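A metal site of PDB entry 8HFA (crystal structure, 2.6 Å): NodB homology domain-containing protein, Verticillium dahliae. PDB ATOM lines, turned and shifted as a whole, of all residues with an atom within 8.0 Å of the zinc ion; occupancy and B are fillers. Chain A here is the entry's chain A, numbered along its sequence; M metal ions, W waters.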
ATOM      1  N   PHE A  54       5.603 -12.179  14.758  1.00  0.00           N
ATOM      2  CA  PHE A  54       4.714 -13.185  14.178  1.00  0.00           C
ATOM      3  C   PHE A  54       3.274 -12.931  14.596  1.00  0.00           C
ATOM      4  O   PHE A  54       2.964 -12.916  15.788  1.00  0.00           O
ATOM      5  CB  PHE A  54       5.153 -14.585  14.599  1.00  0.00           C
ATOM      6  CG  PHE A  54       6.593 -14.911  14.257  1.00  0.00           C
ATOM      7  CD1 PHE A  54       6.918 -15.482  13.031  1.00  0.00           C
ATOM      8  CD2 PHE A  54       7.621 -14.644  15.153  1.00  0.00           C
ATOM      9  CE1 PHE A  54       8.222 -15.795  12.718  1.00  0.00           C
ATOM     10  CE2 PHE A  54       8.933 -14.942  14.822  1.00  0.00           C
ATOM     11  CZ  PHE A  54       9.232 -15.534  13.601  1.00  0.00           C
ATOM     12  N   ASP A  55       2.383 -12.798  13.608  1.00  0.00           N
ATOM     13  CA  ASP A  55       0.984 -12.455  13.823  1.00  0.00           C
ATOM     14  C   ASP A  55       0.082 -13.679  13.673  1.00  0.00           C
ATOM     15  O   ASP A  55       0.420 -14.665  13.008  1.00  0.00           O
ATOM     16  CB  ASP A  55       0.500 -11.408  12.830  1.00  0.00           C
ATOM     17  CG  ASP A  55       1.052 -10.057  13.126  1.00  0.00           C
ATOM     18  OD1 ASP A  55       1.949  -9.984  13.999  1.00  0.00           O
ATOM     19  OD2 ASP A  55       0.599  -9.077  12.490  1.00  0.00           O
ATOM     20  N   ASP A  56      -1.084 -13.586  14.333  1.00  0.00           N
ATOM     21  CA  ASP A  56      -2.309 -14.367  14.137  1.00  0.00           C
ATOM     22  C   ASP A  56      -2.302 -15.708  14.871  1.00  0.00           C
ATOM     23  O   ASP A  56      -3.267 -16.447  14.767  1.00  0.00           O
ATOM     24  CB  ASP A  56      -2.617 -14.604  12.643  1.00  0.00           C
ATOM     25  CG  ASP A  56      -2.934 -13.319  11.890  1.00  0.00           C
ATOM     26  OD1 ASP A  56      -3.134 -12.258  12.506  1.00  0.00           O
ATOM     27  OD2 ASP A  56      -2.993 -13.344  10.652  1.00  0.00           O
ATOM     28  N   GLY A  57      -1.264 -16.023  15.646  1.00  0.00           N
ATOM     29  CA  GLY A  57      -1.246 -17.274  16.378  1.00  0.00           C
ATOM     30  C   GLY A  57      -1.956 -17.139  17.711  1.00  0.00           C
ATOM     31  O   GLY A  57      -2.629 -16.138  17.987  1.00  0.00           O
ATOM     32  N   PHE A  79       2.308 -11.661  18.267  1.00  0.00           N
ATOM     33  CA  PHE A  79       1.062 -10.930  18.450  1.00  0.00           C
ATOM     34  C   PHE A  79      -0.087 -11.896  18.252  1.00  0.00           C
ATOM     35  O   PHE A  79      -0.356 -12.327  17.124  1.00  0.00           O
ATOM     36  CB  PHE A  79       0.989  -9.750  17.492  1.00  0.00           C
ATOM     37  CG  PHE A  79       1.979  -8.660  17.801  1.00  0.00           C
ATOM     38  CD1 PHE A  79       1.707  -7.713  18.777  1.00  0.00           C
ATOM     39  CD2 PHE A  79       3.183  -8.575  17.102  1.00  0.00           C
ATOM     40  CE1 PHE A  79       2.620  -6.690  19.055  1.00  0.00           C
ATOM     41  CE2 PHE A  79       4.087  -7.565  17.375  1.00  0.00           C
ATOM     42  CZ  PHE A  79       3.799  -6.614  18.348  1.00  0.00           C
ATOM     43  N   ASN A  81      -4.070 -13.692  18.880  1.00  0.00           N
ATOM     44  CA  ASN A  81      -5.506 -13.453  19.044  1.00  0.00           C
ATOM     45  C   ASN A  81      -6.052 -14.395  20.105  1.00  0.00           C
ATOM     46  O   ASN A  81      -5.506 -15.464  20.377  1.00  0.00           O
ATOM     47  CB  ASN A  81      -6.267 -13.667  17.720  1.00  0.00           C
ATOM     48  CG  ASN A  81      -5.709 -12.848  16.551  1.00  0.00           C
ATOM     49  OD1 ASN A  81      -5.140 -13.415  15.613  1.00  0.00           O
ATOM     50  ND2 ASN A  81      -5.884 -11.529  16.599  1.00  0.00           N
ATOM     51  N   ASN A  84      -8.751 -17.366  16.727  1.00  0.00           N
ATOM     52  CA  ASN A  84      -8.587 -17.152  15.284  1.00  0.00           C
ATOM     53  C   ASN A  84      -8.285 -18.466  14.579  1.00  0.00           C
ATOM     54  O   ASN A  84      -9.210 -19.158  14.138  1.00  0.00           O
ATOM     55  CB  ASN A  84      -7.491 -16.106  15.033  1.00  0.00           C
ATOM     56  CG  ASN A  84      -7.441 -15.654  13.584  1.00  0.00           C
ATOM     57  OD1 ASN A  84      -8.099 -16.229  12.720  1.00  0.00           O
ATOM     58  ND2 ASN A  84      -6.667 -14.604  13.316  1.00  0.00           N
ATOM     59  N   PHE A  85      -7.007 -18.841  14.469  1.00  0.00           N
ATOM     60  CA  PHE A  85      -6.657 -20.183  13.993  1.00  0.00           C
ATOM     61  C   PHE A  85      -6.713 -21.181  15.131  1.00  0.00           C
ATOM     62  O   PHE A  85      -7.348 -22.240  15.024  1.00  0.00           O
ATOM     63  CB  PHE A  85      -5.269 -20.176  13.338  1.00  0.00           C
ATOM     64  CG  PHE A  85      -5.212 -19.427  12.028  1.00  0.00           C
ATOM     65  CD1 PHE A  85      -5.157 -18.040  12.011  1.00  0.00           C
ATOM     66  CD2 PHE A  85      -5.219 -20.119  10.825  1.00  0.00           C
ATOM     67  CE1 PHE A  85      -5.117 -17.349  10.797  1.00  0.00           C
ATOM     68  CE2 PHE A  85      -5.179 -19.428   9.611  1.00  0.00           C
ATOM     69  CZ  PHE A  85      -5.132 -18.045   9.599  1.00  0.00           C
ATOM     70  N   HIS A 108      -3.002  -8.989  19.504  1.00  0.00           N
ATOM     71  CA  HIS A 108      -3.511  -8.811  18.151  1.00  0.00           C
ATOM     72  C   HIS A 108      -5.049  -8.771  18.128  1.00  0.00           C
ATOM     73  O   HIS A 108      -5.652  -9.096  17.094  1.00  0.00           O
ATOM     74  CB  HIS A 108      -2.967  -9.923  17.247  1.00  0.00           C
ATOM     75  CG  HIS A 108      -2.895  -9.559  15.794  1.00  0.00           C
ATOM     76  ND1 HIS A 108      -2.684  -8.276  15.345  1.00  0.00           N
ATOM     77  CD2 HIS A 108      -2.987 -10.334  14.681  1.00  0.00           C
ATOM     78  CE1 HIS A 108      -2.661  -8.263  14.023  1.00  0.00           C
ATOM     79  NE2 HIS A 108      -2.850  -9.502  13.583  1.00  0.00           N
ATOM     80  N   THR A 109      -5.671  -8.403  19.252  1.00  0.00           N
ATOM     81  CA  THR A 109      -7.123  -8.342  19.534  1.00  0.00           C
ATOM     82  C   THR A 109      -7.709  -9.736  19.754  1.00  0.00           C
ATOM     83  O   THR A 109      -7.047 -10.754  19.509  1.00  0.00           O
ATOM     84  CB  THR A 109      -7.947  -7.630  18.441  1.00  0.00           C
ATOM     85  OG1 THR A 109      -7.969  -8.424  17.246  1.00  0.00           O
ATOM     86  CG2 THR A 109      -7.431  -6.222  18.156  1.00  0.00           C
ATOM     87  N   HIS A 112      -9.649 -10.703  15.691  1.00  0.00           N
ATOM     88  CA  HIS A 112      -9.099 -10.219  14.421  1.00  0.00           C
ATOM     89  C   HIS A 112     -10.112  -9.500  13.535  1.00  0.00           C
ATOM     90  O   HIS A 112     -10.286  -9.882  12.372  1.00  0.00           O
ATOM     91  CB  HIS A 112      -8.489 -11.395  13.646  1.00  0.00           C
ATOM     92  CG  HIS A 112      -7.364 -11.008  12.733  1.00  0.00           C
ATOM     93  ND1 HIS A 112      -7.478 -11.028  11.364  1.00  0.00           N
ATOM     94  CD2 HIS A 112      -6.106 -10.574  12.991  1.00  0.00           C
ATOM     95  CE1 HIS A 112      -6.337 -10.630  10.818  1.00  0.00           C
ATOM     96  NE2 HIS A 112      -5.493 -10.361  11.781  1.00  0.00           N
ATOM     97  N   PRO A 113     -10.770  -8.450  14.016  1.00  0.00           N
ATOM     98  CA  PRO A 113     -11.627  -7.646  13.162  1.00  0.00           C
ATOM     99  C   PRO A 113     -10.854  -6.457  12.571  1.00  0.00           C
ATOM    100  O   PRO A 113      -9.718  -6.185  12.948  1.00  0.00           O
ATOM    101  CB  PRO A 113     -12.699  -7.156  14.133  1.00  0.00           C
ATOM    102  CG  PRO A 113     -11.867  -6.845  15.374  1.00  0.00           C
ATOM    103  CD  PRO A 113     -10.740  -7.895  15.391  1.00  0.00           C
ATOM    104  N   ARG A 146      -0.523  -4.967  18.013  1.00  0.00           N
ATOM    105  CA  ARG A 146      -0.475  -4.679  16.593  1.00  0.00           C
ATOM    106  C   ARG A 146      -1.882  -4.751  16.026  1.00  0.00           C
ATOM    107  O   ARG A 146      -2.558  -5.805  16.147  1.00  0.00           O
ATOM    108  CB  ARG A 146       0.453  -5.649  15.852  1.00  0.00           C
ATOM    109  CG  ARG A 146       0.517  -5.348  14.364  1.00  0.00           C
ATOM    110  CD  ARG A 146       1.496  -6.284  13.671  1.00  0.00           C
ATOM    111  NE  ARG A 146       2.865  -5.805  13.772  1.00  0.00           N
ATOM    112  CZ  ARG A 146       3.920  -6.608  13.839  1.00  0.00           C
ATOM    113  NH1 ARG A 146       3.778  -7.928  13.840  1.00  0.00           N
ATOM    114  NH2 ARG A 146       5.134  -6.074  13.906  1.00  0.00           N
ATOM    115  N   PRO A 147      -2.371  -3.689  15.390  1.00  0.00           N
ATOM    116  CA  PRO A 147      -3.730  -3.693  14.847  1.00  0.00           C
ATOM    117  C   PRO A 147      -3.832  -4.704  13.717  1.00  0.00           C
ATOM    118  O   PRO A 147      -2.958  -4.752  12.847  1.00  0.00           O
ATOM    119  CB  PRO A 147      -3.921  -2.268  14.321  1.00  0.00           C
ATOM    120  CG  PRO A 147      -2.877  -1.452  15.005  1.00  0.00           C
ATOM    121  CD  PRO A 147      -1.719  -2.375  15.245  1.00  0.00           C
ATOM    122  N   PRO A 148      -4.888  -5.527  13.694  1.00  0.00           N
ATOM    123  CA  PRO A 148      -5.069  -6.438  12.564  1.00  0.00           C
ATOM    124  C   PRO A 148      -5.135  -5.678  11.241  1.00  0.00           C
ATOM    125  O   PRO A 148      -5.624  -4.544  11.172  1.00  0.00           O
ATOM    126  CB  PRO A 148      -6.385  -7.143  12.891  1.00  0.00           C
ATOM    127  CG  PRO A 148      -6.425  -7.109  14.426  1.00  0.00           C
ATOM    128  CD  PRO A 148      -5.860  -5.760  14.784  1.00  0.00           C
ATOM    129  N   TYR A 149      -4.561  -6.285  10.201  1.00  0.00           N
ATOM    130  CA  TYR A 149      -4.518  -5.697   8.858  1.00  0.00           C
ATOM    131  C   TYR A 149      -3.877  -4.325   8.839  1.00  0.00           C
ATOM    132  O   TYR A 149      -3.995  -3.606   7.836  1.00  0.00           O
ATOM    133  CB  TYR A 149      -5.922  -5.602   8.227  1.00  0.00           C
ATOM    134  CG  TYR A 149      -6.815  -6.795   8.425  1.00  0.00           C
ATOM    135  CD1 TYR A 149      -6.652  -7.940   7.667  1.00  0.00           C
ATOM    136  CD2 TYR A 149      -7.849  -6.768   9.364  1.00  0.00           C
ATOM    137  CE1 TYR A 149      -7.488  -9.045   7.836  1.00  0.00           C
ATOM    138  CE2 TYR A 149      -8.683  -7.874   9.555  1.00  0.00           C
ATOM    139  CZ  TYR A 149      -8.497  -9.010   8.782  1.00  0.00           C
ATOM    140  OH  TYR A 149      -9.303 -10.104   8.946  1.00  0.00           O
ATOM    141  N   PHE A 150      -3.203  -3.927   9.919  1.00  0.00           N
ATOM    142  CA  PHE A 150      -2.654  -2.560  10.055  1.00  0.00           C
ATOM    143  C   PHE A 150      -3.729  -1.512   9.814  1.00  0.00           C
ATOM    144  O   PHE A 150      -3.457  -0.433   9.282  1.00  0.00           O
ATOM    145  CB  PHE A 150      -1.461  -2.350   9.132  1.00  0.00           C
ATOM    146  CG  PHE A 150      -0.318  -3.251   9.424  1.00  0.00           C
ATOM    147  CD1 PHE A 150       0.392  -3.127  10.601  1.00  0.00           C
ATOM    148  CD2 PHE A 150       0.009  -4.285   8.563  1.00  0.00           C
ATOM    149  CE1 PHE A 150       1.444  -3.986  10.894  1.00  0.00           C
ATOM    150  CE2 PHE A 150       1.044  -5.139   8.853  1.00  0.00           C
ATOM    151  CZ  PHE A 150       1.763  -4.999  10.013  1.00  0.00           C
ATOM    152  N   LEU A 199       7.660  -8.637   9.749  1.00  0.00           N
ATOM    153  CA  LEU A 199       6.315  -9.164   9.903  1.00  0.00           C
ATOM    154  C   LEU A 199       6.200 -10.511   9.203  1.00  0.00           C
ATOM    155  O   LEU A 199       6.483 -10.620   8.001  1.00  0.00           O
ATOM    156  CB  LEU A 199       5.283  -8.195   9.325  1.00  0.00           C
ATOM    157  CG  LEU A 199       3.916  -8.817   8.962  1.00  0.00           C
ATOM    158  CD1 LEU A 199       3.187  -9.404  10.192  1.00  0.00           C
ATOM    159  CD2 LEU A 199       3.035  -7.799   8.215  1.00  0.00           C
ATOM    160  N   ALA A 200       5.786 -11.524   9.956  1.00  0.00           N
ATOM    161  CA  ALA A 200       5.454 -12.822   9.383  1.00  0.00           C
ATOM    162  C   ALA A 200       4.209 -13.348  10.079  1.00  0.00           C
ATOM    163  O   ALA A 200       3.639 -12.680  10.961  1.00  0.00           O
ATOM    164  CB  ALA A 200       6.624 -13.793   9.506  1.00  0.00           C
ATOM    165  N   HIS A 201       3.718 -14.504   9.649  1.00  0.00           N
ATOM    166  CA  HIS A 201       2.508 -15.089  10.217  1.00  0.00           C
ATOM    167  C   HIS A 201       2.798 -16.553  10.531  1.00  0.00           C
ATOM    168  O   HIS A 201       2.820 -17.393   9.625  1.00  0.00           O
ATOM    169  CB  HIS A 201       1.336 -14.911   9.265  1.00  0.00           C
ATOM    170  CG  HIS A 201       1.018 -13.478   8.946  1.00  0.00           C
ATOM    171  ND1 HIS A 201       1.802 -12.708   8.103  1.00  0.00           N
ATOM    172  CD2 HIS A 201       0.026 -12.659   9.370  1.00  0.00           C
ATOM    173  CE1 HIS A 201       1.293 -11.494   8.015  1.00  0.00           C
ATOM    174  NE2 HIS A 201       0.214 -11.434   8.779  1.00  0.00           N
ATOM    175  N   VAL A 203       1.083 -18.800  11.724  1.00  0.00           N
ATOM    176  CA  VAL A 203       0.003 -19.773  11.511  1.00  0.00           C
ATOM    177  C   VAL A 203       0.143 -20.542  10.212  1.00  0.00           C
ATOM    178  O   VAL A 203      -0.512 -21.592  10.058  1.00  0.00           O
ATOM    179  CB  VAL A 203      -1.369 -19.070  11.527  1.00  0.00           C
ATOM    180  CG1 VAL A 203      -1.677 -18.575  12.934  1.00  0.00           C
ATOM    181  CG2 VAL A 203      -1.396 -17.944  10.525  1.00  0.00           C
HETATM  182 ZN    ZN M   1      -3.189 -10.277  11.391  1.00  0.00          ZN
HETATM  183  O   HOH W   1      -1.941  -8.293  10.620  1.00  0.00           O
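ND1 of His 112 is in hydrogen-bond range of OH of Tyr 149.
ND1 of His 108 sits at hydrogen-bond distance from O of Arg 146 (2.6 Å).
N of His 112 sits at hydrogen-bond distance from OG1 of Thr 109 (3.2 Å).
O of Phe 79 is in hydrogen-bond range of N of Asp 56.
The side-chain amide nitrogen of Asn 81 is in hydrogen-bond range of the backbone carbonyl oxygen of His 108 (2.5 Å).
The nearest printed residue that does not touch the zinc ion is Asp 55 (4.1 Å).
The zinc ion is bound by the side-chain carboxylate (OD1) of Asp 56, 2.3 Å away.
The zinc ion is bound by NE2 of His 112, 2.3 Å away.
The zinc ion is bound by NE2 of His 108 (2.3 Å).
Water W1 is bound to the zinc ion.
The zinc ion has four donor atoms within binding distance.
Water W1 lies within hydrogen-bond range of OD2 of Asp 55 and N of Tyr 149.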
